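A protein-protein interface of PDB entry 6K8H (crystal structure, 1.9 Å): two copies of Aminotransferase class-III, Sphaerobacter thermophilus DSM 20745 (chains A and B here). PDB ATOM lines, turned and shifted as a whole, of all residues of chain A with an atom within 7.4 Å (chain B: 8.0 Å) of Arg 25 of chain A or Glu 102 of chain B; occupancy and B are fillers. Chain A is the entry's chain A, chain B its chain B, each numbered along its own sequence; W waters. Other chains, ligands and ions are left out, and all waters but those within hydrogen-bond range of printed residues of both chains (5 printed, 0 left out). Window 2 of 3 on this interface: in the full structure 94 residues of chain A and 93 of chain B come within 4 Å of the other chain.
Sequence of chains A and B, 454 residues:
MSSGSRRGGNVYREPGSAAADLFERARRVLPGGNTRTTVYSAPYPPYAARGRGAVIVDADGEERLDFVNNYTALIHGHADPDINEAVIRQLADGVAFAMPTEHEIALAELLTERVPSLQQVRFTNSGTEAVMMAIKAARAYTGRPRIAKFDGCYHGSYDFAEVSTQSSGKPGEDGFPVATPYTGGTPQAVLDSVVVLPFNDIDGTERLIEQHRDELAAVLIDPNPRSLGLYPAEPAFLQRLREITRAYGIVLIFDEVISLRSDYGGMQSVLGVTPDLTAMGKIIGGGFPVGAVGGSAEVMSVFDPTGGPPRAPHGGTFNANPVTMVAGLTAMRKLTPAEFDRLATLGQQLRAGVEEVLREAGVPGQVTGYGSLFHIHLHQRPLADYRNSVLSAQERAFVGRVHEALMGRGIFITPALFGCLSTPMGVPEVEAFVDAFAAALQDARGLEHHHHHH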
ATOM      1  N   ALA A  19      -2.952 -15.607  31.987  1.00  0.00           N
ATOM      2  CA  ALA A  19      -1.725 -15.739  31.206  1.00  0.00           C
ATOM      3  C   ALA A  19      -0.528 -16.033  32.097  1.00  0.00           C
ATOM      4  O   ALA A  19       0.343 -16.831  31.729  1.00  0.00           O
ATOM      5  CB  ALA A  19      -1.465 -14.473  30.389  1.00  0.00           C
ATOM      6  N   ALA A  20      -0.467 -15.403  33.275  1.00  0.00           N
ATOM      7  CA  ALA A  20       0.658 -15.641  34.174  1.00  0.00           C
ATOM      8  C   ALA A  20       0.682 -17.084  34.672  1.00  0.00           C
ATOM      9  O   ALA A  20       1.750 -17.712  34.721  1.00  0.00           O
ATOM     10  CB  ALA A  20       0.602 -14.669  35.354  1.00  0.00           C
ATOM     11  N   ASP A  21      -0.487 -17.624  35.055  1.00  0.00           N
ATOM     12  CA  ASP A  21      -0.561 -19.017  35.509  1.00  0.00           C
ATOM     13  C   ASP A  21      -0.202 -19.981  34.388  1.00  0.00           C
ATOM     14  O   ASP A  21       0.517 -20.973  34.599  1.00  0.00           O
ATOM     15  CB  ASP A  21      -1.965 -19.341  36.027  1.00  0.00           C
ATOM     16  CG  ASP A  21      -2.312 -18.615  37.311  1.00  0.00           C
ATOM     17  OD1 ASP A  21      -1.440 -17.944  37.896  1.00  0.00           O
ATOM     18  OD2 ASP A  21      -3.480 -18.724  37.738  1.00  0.00           O
ATOM     19  N   LEU A  22      -0.732 -19.728  33.190  1.00  0.00           N
ATOM     20  CA  LEU A  22      -0.402 -20.578  32.056  1.00  0.00           C
ATOM     21  C   LEU A  22       1.093 -20.561  31.765  1.00  0.00           C
ATOM     22  O   LEU A  22       1.689 -21.617  31.538  1.00  0.00           O
ATOM     23  CB  LEU A  22      -1.203 -20.141  30.832  1.00  0.00           C
ATOM     24  CG  LEU A  22      -2.702 -20.416  30.931  1.00  0.00           C
ATOM     25  CD1 LEU A  22      -3.448 -19.622  29.871  1.00  0.00           C
ATOM     26  CD2 LEU A  22      -2.999 -21.906  30.787  1.00  0.00           C
ATOM     27  N   PHE A  23       1.719 -19.376  31.778  1.00  0.00           N
ATOM     28  CA  PHE A  23       3.162 -19.288  31.545  1.00  0.00           C
ATOM     29  C   PHE A  23       3.935 -20.047  32.617  1.00  0.00           C
ATOM     30  O   PHE A  23       4.939 -20.707  32.323  1.00  0.00           O
ATOM     31  CB  PHE A  23       3.586 -17.822  31.493  1.00  0.00           C
ATOM     32  CG  PHE A  23       5.068 -17.603  31.309  1.00  0.00           C
ATOM     33  CD1 PHE A  23       5.673 -17.807  30.077  1.00  0.00           C
ATOM     34  CD2 PHE A  23       5.849 -17.153  32.362  1.00  0.00           C
ATOM     35  CE1 PHE A  23       7.043 -17.584  29.906  1.00  0.00           C
ATOM     36  CE2 PHE A  23       7.212 -16.927  32.203  1.00  0.00           C
ATOM     37  CZ  PHE A  23       7.812 -17.151  30.969  1.00  0.00           C
ATOM     38  N   GLU A  24       3.479 -19.968  33.869  1.00  0.00           N
ATOM     39  CA  GLU A  24       4.136 -20.724  34.927  1.00  0.00           C
ATOM     40  C   GLU A  24       4.098 -22.220  34.629  1.00  0.00           C
ATOM     41  O   GLU A  24       5.099 -22.917  34.824  1.00  0.00           O
ATOM     42  CB  GLU A  24       3.479 -20.424  36.274  1.00  0.00           C
ATOM     43  CG  GLU A  24       4.200 -21.013  37.463  1.00  0.00           C
ATOM     44  CD  GLU A  24       3.565 -20.607  38.783  1.00  0.00           C
ATOM     45  OE1 GLU A  24       2.321 -20.474  38.831  1.00  0.00           O
ATOM     46  OE2 GLU A  24       4.309 -20.425  39.771  1.00  0.00           O
ATOM     47  N   ARG A  25       2.959 -22.728  34.134  1.00  0.00           N
ATOM     48  CA  ARG A  25       2.911 -24.129  33.701  1.00  0.00           C
ATOM     49  C   ARG A  25       3.828 -24.379  32.503  1.00  0.00           C
ATOM     50  O   ARG A  25       4.555 -25.379  32.449  1.00  0.00           O
ATOM     51  CB  ARG A  25       1.480 -24.534  33.330  1.00  0.00           C
ATOM     52  CG  ARG A  25       0.561 -24.874  34.476  1.00  0.00           C
ATOM     53  CD  ARG A  25      -0.855 -25.099  33.968  1.00  0.00           C
ATOM     54  NE  ARG A  25      -0.958 -26.217  33.032  1.00  0.00           N
ATOM     55  CZ  ARG A  25      -2.012 -26.426  32.242  1.00  0.00           C
ATOM     56  NH1 ARG A  25      -3.037 -25.587  32.278  1.00  0.00           N
ATOM     57  NH2 ARG A  25      -2.050 -27.468  31.421  1.00  0.00           N
ATOM     58  N   ALA A  26       3.772 -23.487  31.516  1.00  0.00           N
ATOM     59  CA  ALA A  26       4.451 -23.703  30.247  1.00  0.00           C
ATOM     60  C   ALA A  26       5.951 -23.805  30.432  1.00  0.00           C
ATOM     61  O   ALA A  26       6.601 -24.645  29.799  1.00  0.00           O
ATOM     62  CB  ALA A  26       4.113 -22.575  29.274  1.00  0.00           C
ATOM     63  N   ARG A  27       6.525 -22.953  31.290  1.00  0.00           N
ATOM     64  CA  ARG A  27       7.983 -22.932  31.368  1.00  0.00           C
ATOM     65  C   ARG A  27       8.559 -24.199  31.992  1.00  0.00           C
ATOM     66  O   ARG A  27       9.772 -24.406  31.911  1.00  0.00           O
ATOM     67  CB  ARG A  27       8.473 -21.685  32.117  1.00  0.00           C
ATOM     68  CG  ARG A  27       8.096 -21.591  33.578  1.00  0.00           C
ATOM     69  CD  ARG A  27       8.284 -20.144  34.104  1.00  0.00           C
ATOM     70  NE  ARG A  27       9.688 -19.762  34.244  1.00  0.00           N
ATOM     71  CZ  ARG A  27      10.512 -20.213  35.193  1.00  0.00           C
ATOM     72  NH1 ARG A  27      10.085 -21.083  36.106  1.00  0.00           N
ATOM     73  NH2 ARG A  27      11.776 -19.796  35.230  1.00  0.00           N
ATOM     74  N   ARG A  28       7.724 -25.059  32.586  1.00  0.00           N
ATOM     75  CA  ARG A  28       8.214 -26.334  33.087  1.00  0.00           C
ATOM     76  C   ARG A  28       8.359 -27.375  31.977  1.00  0.00           C
ATOM     77  O   ARG A  28       9.171 -28.298  32.102  1.00  0.00           O
ATOM     78  CB  ARG A  28       7.289 -26.844  34.199  1.00  0.00           C
ATOM     79  CG  ARG A  28       7.267 -25.917  35.404  1.00  0.00           C
ATOM     80  CD  ARG A  28       6.686 -26.563  36.643  1.00  0.00           C
ATOM     81  NE  ARG A  28       5.367 -27.114  36.380  1.00  0.00           N
ATOM     82  CZ  ARG A  28       4.231 -26.528  36.748  1.00  0.00           C
ATOM     83  NH1 ARG A  28       4.265 -25.364  37.399  1.00  0.00           N
ATOM     84  NH2 ARG A  28       3.065 -27.108  36.459  1.00  0.00           N
ATOM     85  N   VAL A  29       7.586 -27.263  30.899  1.00  0.00           N
ATOM     86  CA  VAL A  29       7.552 -28.298  29.871  1.00  0.00           C
ATOM     87  C   VAL A  29       7.894 -27.777  28.483  1.00  0.00           C
ATOM     88  O   VAL A  29       8.023 -28.588  27.555  1.00  0.00           O
ATOM     89  CB  VAL A  29       6.187 -29.020  29.840  1.00  0.00           C
ATOM     90  CG1 VAL A  29       5.986 -29.825  31.112  1.00  0.00           C
ATOM     91  CG2 VAL A  29       5.066 -28.026  29.647  1.00  0.00           C
ATOM     92  N   LEU A  30       8.063 -26.468  28.308  1.00  0.00           N
ATOM     93  CA  LEU A  30       8.544 -25.860  27.075  1.00  0.00           C
ATOM     94  C   LEU A  30       9.661 -24.887  27.420  1.00  0.00           C
ATOM     95  O   LEU A  30       9.594 -24.211  28.457  1.00  0.00           O
ATOM     96  CB  LEU A  30       7.425 -25.106  26.339  1.00  0.00           C
ATOM     97  CG  LEU A  30       6.116 -25.874  26.112  1.00  0.00           C
ATOM     98  CD1 LEU A  30       4.926 -24.948  26.337  1.00  0.00           C
ATOM     99  CD2 LEU A  30       6.062 -26.459  24.707  1.00  0.00           C
ATOM    100  N   GLY A  33       8.886 -21.501  28.303  1.00  0.00           N
ATOM    101  CA  GLY A  33       7.450 -21.529  28.074  1.00  0.00           C
ATOM    102  C   GLY A  33       7.029 -21.307  26.639  1.00  0.00           C
ATOM    103  O   GLY A  33       5.891 -20.895  26.397  1.00  0.00           O
ATOM    104  N   TYR A  47      -2.271 -15.285  26.231  1.00  0.00           N
ATOM    105  CA  TYR A  47      -2.676 -16.577  25.685  1.00  0.00           C
ATOM    106  C   TYR A  47      -4.046 -16.445  25.036  1.00  0.00           C
ATOM    107  O   TYR A  47      -4.952 -15.843  25.623  1.00  0.00           O
ATOM    108  CB  TYR A  47      -2.720 -17.663  26.767  1.00  0.00           C
ATOM    109  CG  TYR A  47      -1.364 -18.244  27.072  1.00  0.00           C
ATOM    110  CD1 TYR A  47      -0.410 -17.493  27.732  1.00  0.00           C
ATOM    111  CD2 TYR A  47      -1.036 -19.544  26.695  1.00  0.00           C
ATOM    112  CE1 TYR A  47       0.838 -18.002  28.007  1.00  0.00           C
ATOM    113  CE2 TYR A  47       0.214 -20.071  26.974  1.00  0.00           C
ATOM    114  CZ  TYR A  47       1.146 -19.290  27.629  1.00  0.00           C
ATOM    115  OH  TYR A  47       2.394 -19.784  27.916  1.00  0.00           O
ATOM    116  N   ALA A  48      -4.189 -17.005  23.832  1.00  0.00           N
ATOM    117  CA  ALA A  48      -5.471 -17.015  23.136  1.00  0.00           C
ATOM    118  C   ALA A  48      -6.380 -18.076  23.737  1.00  0.00           C
ATOM    119  O   ALA A  48      -5.948 -19.209  23.976  1.00  0.00           O
ATOM    120  CB  ALA A  48      -5.278 -17.298  21.641  1.00  0.00           C
ATOM    121  N   ALA A  49      -7.642 -17.711  23.973  1.00  0.00           N
ATOM    122  CA  ALA A  49      -8.660 -18.667  24.386  1.00  0.00           C
ATOM    123  C   ALA A  49      -9.527 -19.094  23.212  1.00  0.00           C
ATOM    124  O   ALA A  49      -9.781 -20.290  23.020  1.00  0.00           O
ATOM    125  CB  ALA A  49      -9.548 -18.080  25.488  1.00  0.00           C
ATOM    126  N   ALA A  59      -6.971 -15.459  27.304  1.00  0.00           N
ATOM    127  CA  ALA A  59      -7.338 -16.302  28.435  1.00  0.00           C
ATOM    128  C   ALA A  59      -7.878 -15.502  29.611  1.00  0.00           C
ATOM    129  O   ALA A  59      -8.551 -16.079  30.472  1.00  0.00           O
ATOM    130  CB  ALA A  59      -6.136 -17.140  28.879  1.00  0.00           C
ATOM    131  N   MET B  99      -1.037 -16.211  19.184  1.00  0.00           N
ATOM    132  CA  MET B  99      -0.697 -16.282  20.594  1.00  0.00           C
ATOM    133  C   MET B  99      -0.568 -17.751  20.957  1.00  0.00           C
ATOM    134  O   MET B  99      -1.186 -18.599  20.301  1.00  0.00           O
ATOM    135  CB  MET B  99      -1.774 -15.644  21.481  1.00  0.00           C
ATOM    136  CG  MET B  99      -2.130 -14.207  21.174  1.00  0.00           C
ATOM    137  SD  MET B  99      -3.530 -13.697  22.208  1.00  0.00           S
ATOM    138  CE  MET B  99      -3.819 -12.032  21.581  1.00  0.00           C
ATOM    139  N   PRO B 100       0.218 -18.089  21.983  1.00  0.00           N
ATOM    140  CA  PRO B 100       0.203 -19.469  22.495  1.00  0.00           C
ATOM    141  C   PRO B 100      -1.163 -19.807  23.082  1.00  0.00           C
ATOM    142  O   PRO B 100      -1.969 -18.928  23.387  1.00  0.00           O
ATOM    143  CB  PRO B 100       1.294 -19.462  23.579  1.00  0.00           C
ATOM    144  CG  PRO B 100       1.337 -17.993  24.041  1.00  0.00           C
ATOM    145  CD  PRO B 100       1.127 -17.219  22.759  1.00  0.00           C
ATOM    146  N   THR B 101      -1.410 -21.105  23.242  1.00  0.00           N
ATOM    147  CA  THR B 101      -2.685 -21.566  23.835  1.00  0.00           C
ATOM    148  C   THR B 101      -2.389 -22.653  24.865  1.00  0.00           C
ATOM    149  O   THR B 101      -1.318 -23.267  24.798  1.00  0.00           O
ATOM    150  CB  THR B 101      -3.664 -22.121  22.794  1.00  0.00           C
ATOM    151  OG1 THR B 101      -3.354 -23.488  22.535  1.00  0.00           O
ATOM    152  CG2 THR B 101      -3.699 -21.317  21.514  1.00  0.00           C
ATOM    153  N   GLU B 102      -3.313 -22.839  25.797  1.00  0.00           N
ATOM    154  CA  GLU B 102      -3.175 -23.876  26.811  1.00  0.00           C
ATOM    155  C   GLU B 102      -3.033 -25.269  26.196  1.00  0.00           C
ATOM    156  O   GLU B 102      -2.489 -26.171  26.843  1.00  0.00           O
ATOM    157  CB  GLU B 102      -4.382 -23.818  27.749  1.00  0.00           C
ATOM    158  CG  GLU B 102      -4.351 -24.804  28.919  1.00  0.00           C
ATOM    159  CD  GLU B 102      -5.516 -24.595  29.874  1.00  0.00           C
ATOM    160  OE1 GLU B 102      -6.276 -23.618  29.676  1.00  0.00           O
ATOM    161  OE2 GLU B 102      -5.666 -25.399  30.826  1.00  0.00           O
ATOM    162  N   HIS B 103      -3.513 -25.466  24.959  1.00  0.00           N
ATOM    163  CA  HIS B 103      -3.489 -26.799  24.354  1.00  0.00           C
ATOM    164  C   HIS B 103      -2.062 -27.305  24.158  1.00  0.00           C
ATOM    165  O   HIS B 103      -1.782 -28.499  24.361  1.00  0.00           O
ATOM    166  CB  HIS B 103      -4.246 -26.771  23.020  1.00  0.00           C
ATOM    167  CG  HIS B 103      -5.627 -26.199  23.118  1.00  0.00           C
ATOM    168  ND1 HIS B 103      -6.684 -26.892  23.671  1.00  0.00           N
ATOM    169  CD2 HIS B 103      -6.125 -24.999  22.734  1.00  0.00           C
ATOM    170  CE1 HIS B 103      -7.774 -26.148  23.615  1.00  0.00           C
ATOM    171  NE2 HIS B 103      -7.463 -24.992  23.055  1.00  0.00           N
ATOM    172  N   GLU B 104      -1.158 -26.394  23.789  1.00  0.00           N
ATOM    173  CA  GLU B 104       0.272 -26.761  23.607  1.00  0.00           C
ATOM    174  C   GLU B 104       0.823 -27.215  24.964  1.00  0.00           C
ATOM    175  O   GLU B 104       1.577 -28.174  25.004  1.00  0.00           O
ATOM    176  CB  GLU B 104       1.067 -25.604  22.995  1.00  0.00           C
ATOM    177  CG  GLU B 104       1.273 -24.422  23.914  1.00  0.00           C
ATOM    178  CD  GLU B 104       1.823 -23.175  23.233  1.00  0.00           C
ATOM    179  OE1 GLU B 104       1.291 -22.803  22.175  1.00  0.00           O
ATOM    180  OE2 GLU B 104       2.782 -22.592  23.767  1.00  0.00           O
ATOM    181  N   ILE B 105       0.428 -26.539  26.040  1.00  0.00           N
ATOM    182  CA  ILE B 105       0.882 -26.929  27.373  1.00  0.00           C
ATOM    183  C   ILE B 105       0.375 -28.315  27.718  1.00  0.00           C
ATOM    184  O   ILE B 105       1.101 -29.125  28.299  1.00  0.00           O
ATOM    185  CB  ILE B 105       0.434 -25.904  28.428  1.00  0.00           C
ATOM    186  CG1 ILE B 105       0.911 -24.507  28.034  1.00  0.00           C
ATOM    187  CG2 ILE B 105       0.982 -26.318  29.806  1.00  0.00           C
ATOM    188  CD1 ILE B 105       0.408 -23.407  28.947  1.00  0.00           C
ATOM    189  N   ALA B 106      -0.891 -28.599  27.402  1.00  0.00           N
ATOM    190  CA  ALA B 106      -1.472 -29.891  27.762  1.00  0.00           C
ATOM    191  C   ALA B 106      -0.734 -31.039  27.075  1.00  0.00           C
ATOM    192  O   ALA B 106      -0.364 -32.041  27.718  1.00  0.00           O
ATOM    193  CB  ALA B 106      -2.955 -29.906  27.393  1.00  0.00           C
ATOM    194  N   LEU B 107      -0.477 -30.898  25.764  1.00  0.00           N
ATOM    195  CA  LEU B 107       0.232 -31.972  25.065  1.00  0.00           C
ATOM    196  C   LEU B 107       1.680 -32.093  25.539  1.00  0.00           C
ATOM    197  O   LEU B 107       2.203 -33.212  25.675  1.00  0.00           O
ATOM    198  CB  LEU B 107       0.178 -31.773  23.548  1.00  0.00           C
ATOM    199  CG  LEU B 107       0.694 -32.986  22.760  1.00  0.00           C
ATOM    200  CD1 LEU B 107       0.078 -34.295  23.271  1.00  0.00           C
ATOM    201  CD2 LEU B 107       0.440 -32.852  21.245  1.00  0.00           C
ATOM    202  N   ALA B 108       2.357 -30.962  25.776  1.00  0.00           N
ATOM    203  CA  ALA B 108       3.715 -31.024  26.302  1.00  0.00           C
ATOM    204  C   ALA B 108       3.754 -31.703  27.672  1.00  0.00           C
ATOM    205  O   ALA B 108       4.673 -32.485  27.962  1.00  0.00           O
ATOM    206  CB  ALA B 108       4.310 -29.615  26.358  1.00  0.00           C
ATOM    207  N   GLU B 109       2.767 -31.418  28.530  1.00  0.00           N
ATOM    208  CA  GLU B 109       2.691 -32.076  29.830  1.00  0.00           C
ATOM    209  C   GLU B 109       2.557 -33.592  29.674  1.00  0.00           C
ATOM    210  O   GLU B 109       3.251 -34.360  30.355  1.00  0.00           O
ATOM    211  CB  GLU B 109       1.536 -31.482  30.642  1.00  0.00           C
ATOM    212  CG  GLU B 109       1.944 -30.216  31.421  1.00  0.00           C
ATOM    213  CD  GLU B 109       0.762 -29.391  31.936  1.00  0.00           C
ATOM    214  OE1 GLU B 109      -0.400 -29.712  31.605  1.00  0.00           O
ATOM    215  OE2 GLU B 109       1.007 -28.405  32.666  1.00  0.00           O
ATOM    216  N   ALA B 320       2.204 -25.855  16.987  1.00  0.00           N
ATOM    217  CA  ALA B 320       1.333 -25.970  18.158  1.00  0.00           C
ATOM    218  C   ALA B 320      -0.057 -25.386  17.895  1.00  0.00           C
ATOM    219  O   ALA B 320      -0.718 -24.897  18.811  1.00  0.00           O
ATOM    220  CB  ALA B 320       1.968 -25.322  19.394  1.00  0.00           C
ATOM    221  N   PRO B 322      -3.961 -25.287  17.664  1.00  0.00           N
ATOM    222  CA  PRO B 322      -4.823 -26.022  18.607  1.00  0.00           C
ATOM    223  C   PRO B 322      -5.474 -27.262  18.015  1.00  0.00           C
ATOM    224  O   PRO B 322      -5.769 -28.200  18.760  1.00  0.00           O
ATOM    225  CB  PRO B 322      -5.869 -24.975  19.011  1.00  0.00           C
ATOM    226  CG  PRO B 322      -5.156 -23.659  18.824  1.00  0.00           C
ATOM    227  CD  PRO B 322      -4.288 -23.854  17.608  1.00  0.00           C
ATOM    228  N   MET B 325      -2.888 -29.912  18.412  1.00  0.00           N
ATOM    229  CA  MET B 325      -2.630 -30.151  19.832  1.00  0.00           C
ATOM    230  C   MET B 325      -3.758 -30.946  20.475  1.00  0.00           C
ATOM    231  O   MET B 325      -3.507 -31.871  21.251  1.00  0.00           O
ATOM    232  CB  MET B 325      -2.423 -28.823  20.564  1.00  0.00           C
ATOM    233  CG  MET B 325      -1.191 -28.055  20.098  1.00  0.00           C
ATOM    234  SD  MET B 325       0.394 -28.867  20.428  1.00  0.00           S
ATOM    235  CE  MET B 325       0.664 -29.775  18.894  1.00  0.00           C
ATOM    236  N   VAL B 326      -5.009 -30.606  20.146  1.00  0.00           N
ATOM    237  CA  VAL B 326      -6.164 -31.295  20.704  1.00  0.00           C
ATOM    238  C   VAL B 326      -6.268 -32.720  20.158  1.00  0.00           C
ATOM    239  O   VAL B 326      -6.512 -33.675  20.910  1.00  0.00           O
ATOM    240  CB  VAL B 326      -7.423 -30.455  20.433  1.00  0.00           C
ATOM    241  CG1 VAL B 326      -8.657 -31.280  20.566  1.00  0.00           C
ATOM    242  CG2 VAL B 326      -7.458 -29.246  21.402  1.00  0.00           C
ATOM    243  N   LEU B 329      -3.493 -34.707  21.814  1.00  0.00           N
ATOM    244  CA  LEU B 329      -3.825 -35.002  23.208  1.00  0.00           C
ATOM    245  C   LEU B 329      -4.814 -36.157  23.304  1.00  0.00           C
ATOM    246  O   LEU B 329      -4.636 -37.078  24.113  1.00  0.00           O
ATOM    247  CB  LEU B 329      -4.386 -33.754  23.900  1.00  0.00           C
ATOM    248  CG  LEU B 329      -4.477 -33.935  25.423  1.00  0.00           C
ATOM    249  CD1 LEU B 329      -3.077 -34.099  26.013  1.00  0.00           C
ATOM    250  CD2 LEU B 329      -5.219 -32.792  26.098  1.00  0.00           C
ATOM    251  N   ARG B 333      -3.952 -39.787  24.838  1.00  0.00           N
ATOM    252  CA  ARG B 333      -4.681 -40.195  26.034  1.00  0.00           C
ATOM    253  C   ARG B 333      -5.367 -41.533  25.837  1.00  0.00           C
ATOM    254  O   ARG B 333      -5.545 -42.280  26.804  1.00  0.00           O
ATOM    255  CB  ARG B 333      -5.717 -39.146  26.439  1.00  0.00           C
ATOM    256  CG  ARG B 333      -5.142 -38.049  27.336  1.00  0.00           C
ATOM    257  CD  ARG B 333      -6.209 -37.022  27.730  1.00  0.00           C
ATOM    258  NE  ARG B 333      -5.601 -35.953  28.522  1.00  0.00           N
ATOM    259  CZ  ARG B 333      -6.207 -34.814  28.845  1.00  0.00           C
ATOM    260  NH1 ARG B 333      -7.452 -34.587  28.437  1.00  0.00           N
ATOM    261  NH2 ARG B 333      -5.563 -33.900  29.572  1.00  0.00           N
HETATM  262  O   HOH W   1      -4.416 -27.945  30.137  1.00  0.00           O
HETATM  263  O   HOH W   2      -9.297 -22.995  21.865  1.00  0.00           O
HETATM  264  O   HOH W   3       3.745 -27.706  33.324  1.00  0.00           O
HETATM  265  O   HOH W   4      -5.061 -20.722  26.179  1.00  0.00           O
HETATM  266  O   HOH W   5       3.266 -21.695  26.173  1.00  0.00           O
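Of the 17 printed residues of chain A, 7 touch a printed residue of chain B.
Printed residues of chain A that touch a printed residue of chain B: Leu 22, Arg 25, Ala 26, Val 29, Leu 30, Tyr 47 and Ala 48.
Hydrophobic or aromatic side chains of chain A that line the printed part of chain B: Leu 22, Ala 26, Val 29, Leu 30, Tyr 47 and Ala 48.
Of the 17 printed residues of chain B, 7 touch a printed residue of chain A.
Hydrophobic or aromatic side chains of chain B within 4 Å of the printed part of chain A: Met 99, Pro 100, Ile 105 and Ala 108.
Along chain B the printed residues that touch a printed residue of chain A span positions 99 to 109.
Among the printed residues, Asp or Glu carboxylates within 4 Å of a Lys or Arg side-chain nitrogen of the other chain: Arg 25 of chain A with Glu 102 of chain B and Arg 25 of chain A with Glu 109 of chain B.
Water W5 lies within hydrogen-bond range of the side-chain carboxylate (OE2) of Glu 104 of chain B (2.6 Å), the side-chain hydroxyl (OH) of Tyr 47 of chain A (2.7 Å) and the backbone carbonyl oxygen (O) of Gly 33 of chain A (2.8 Å).
Water W3 lies within hydrogen-bond range of O of Arg 25 of chain A (2.6 Å), OE2 of Glu 109 of chain B (2.9 Å) and NH2 of Arg 28 of chain A (3.3 Å).
Water W1 lies within hydrogen-bond range of the guanidinium group (NH2) of Arg 25 of chain A and the side-chain carboxylate (OE2) of Glu 102 of chain B.
Water W4 lies within hydrogen-bond range of N of Glu 102 of chain B (2.8 Å) and O of Ala 48 of chain A (2.8 Å).
Water W2 bridges NE2 of His 103 of chain B (3.0 Å) and O of Ala 49 of chain A (3.0 Å).
Among the printed residues, merely in contact across the chains: Tyr 47 of chain A with Pro 100 of chain B (3.4 Å), Leu 22 of chain A with Ile 105 of chain B (3.4 Å), Arg 25 of chain A with Ile 105 of chain B (3.6 Å), Leu 22 of chain A with Glu 102 of chain B (3.7 Å), Val 29 of chain A with Ala 108 of chain B (3.7 Å), Tyr 47 of chain A with Thr 101 of chain B (3.8 Å), Ala 26 of chain A with Ile 105 of chain B (3.8 Å), Tyr 47 of chain A with Ile 105 of chain B (3.9 Å), Ala 48 of chain A with Thr 101 of chain B (3.9 Å), Leu 30 of chain A with Ala 108 of chain B (3.97 Å) and Tyr 47 of chain A with Met 99 of chain B (3.98 Å).
No position is printed for both chains.
Of the 15 pairs that touch across the chains among the printed residues, none has its exchanged pair printed and touching as well.
The side-chain hydroxyl (OG1) of Thr 101 of chain B lies close to the backbone NH (N) of His 103 of chain B.
The backbone NH of Thr 101 of chain B is in hydrogen-bond range of the side-chain carboxylate of Glu 104 of chain B.
O of Tyr 47 of chain A is in hydrogen-bond range of N of Ala 59 of chain A, 2.7 Å away.
Of chain A, only Leu 22 (3.7 Å) and Arg 25 (3.0 Å) come within 4 Å of Glu 102 of chain B.
Of the printed residues of chain A, Pro 100 of chain B touches Tyr 47 (3.4 Å) and Ala 48 (3.0 Å).
Of the printed residues of chain A, Glu 109 of chain B touches Arg 25 (2.8 Å).
Of the printed residues of chain B, Leu 22 of chain A touches Glu 102 (3.7 Å) and Ile 105 (3.4 Å).
His 103 of chain B touches none of the printed residues of chain A.
The nearest residue of chain B that does not touch Arg 25 of chain A is Ala 106 of chain B (4.3 Å).
The guanidinium group of Arg 25 of chain A lies within salt-bridge range of the side-chain carboxylate of Glu 109 of chain B (2.8 Å).
OE2 of Glu 102 of chain B is in salt-bridge range of NH1 of Arg 25 of chain A (3.0 Å).
The backbone NH (N) of Ala 48 of chain A sits close to the side-chain sulfur (SD) of Met 99 of chain B, 3.7 Å away.
The backbone carbonyl oxygen (O) of Pro 100 of chain B lies within hydrogen-bond range of the backbone NH (N) of Ala 48 of chain A (3.0 Å).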
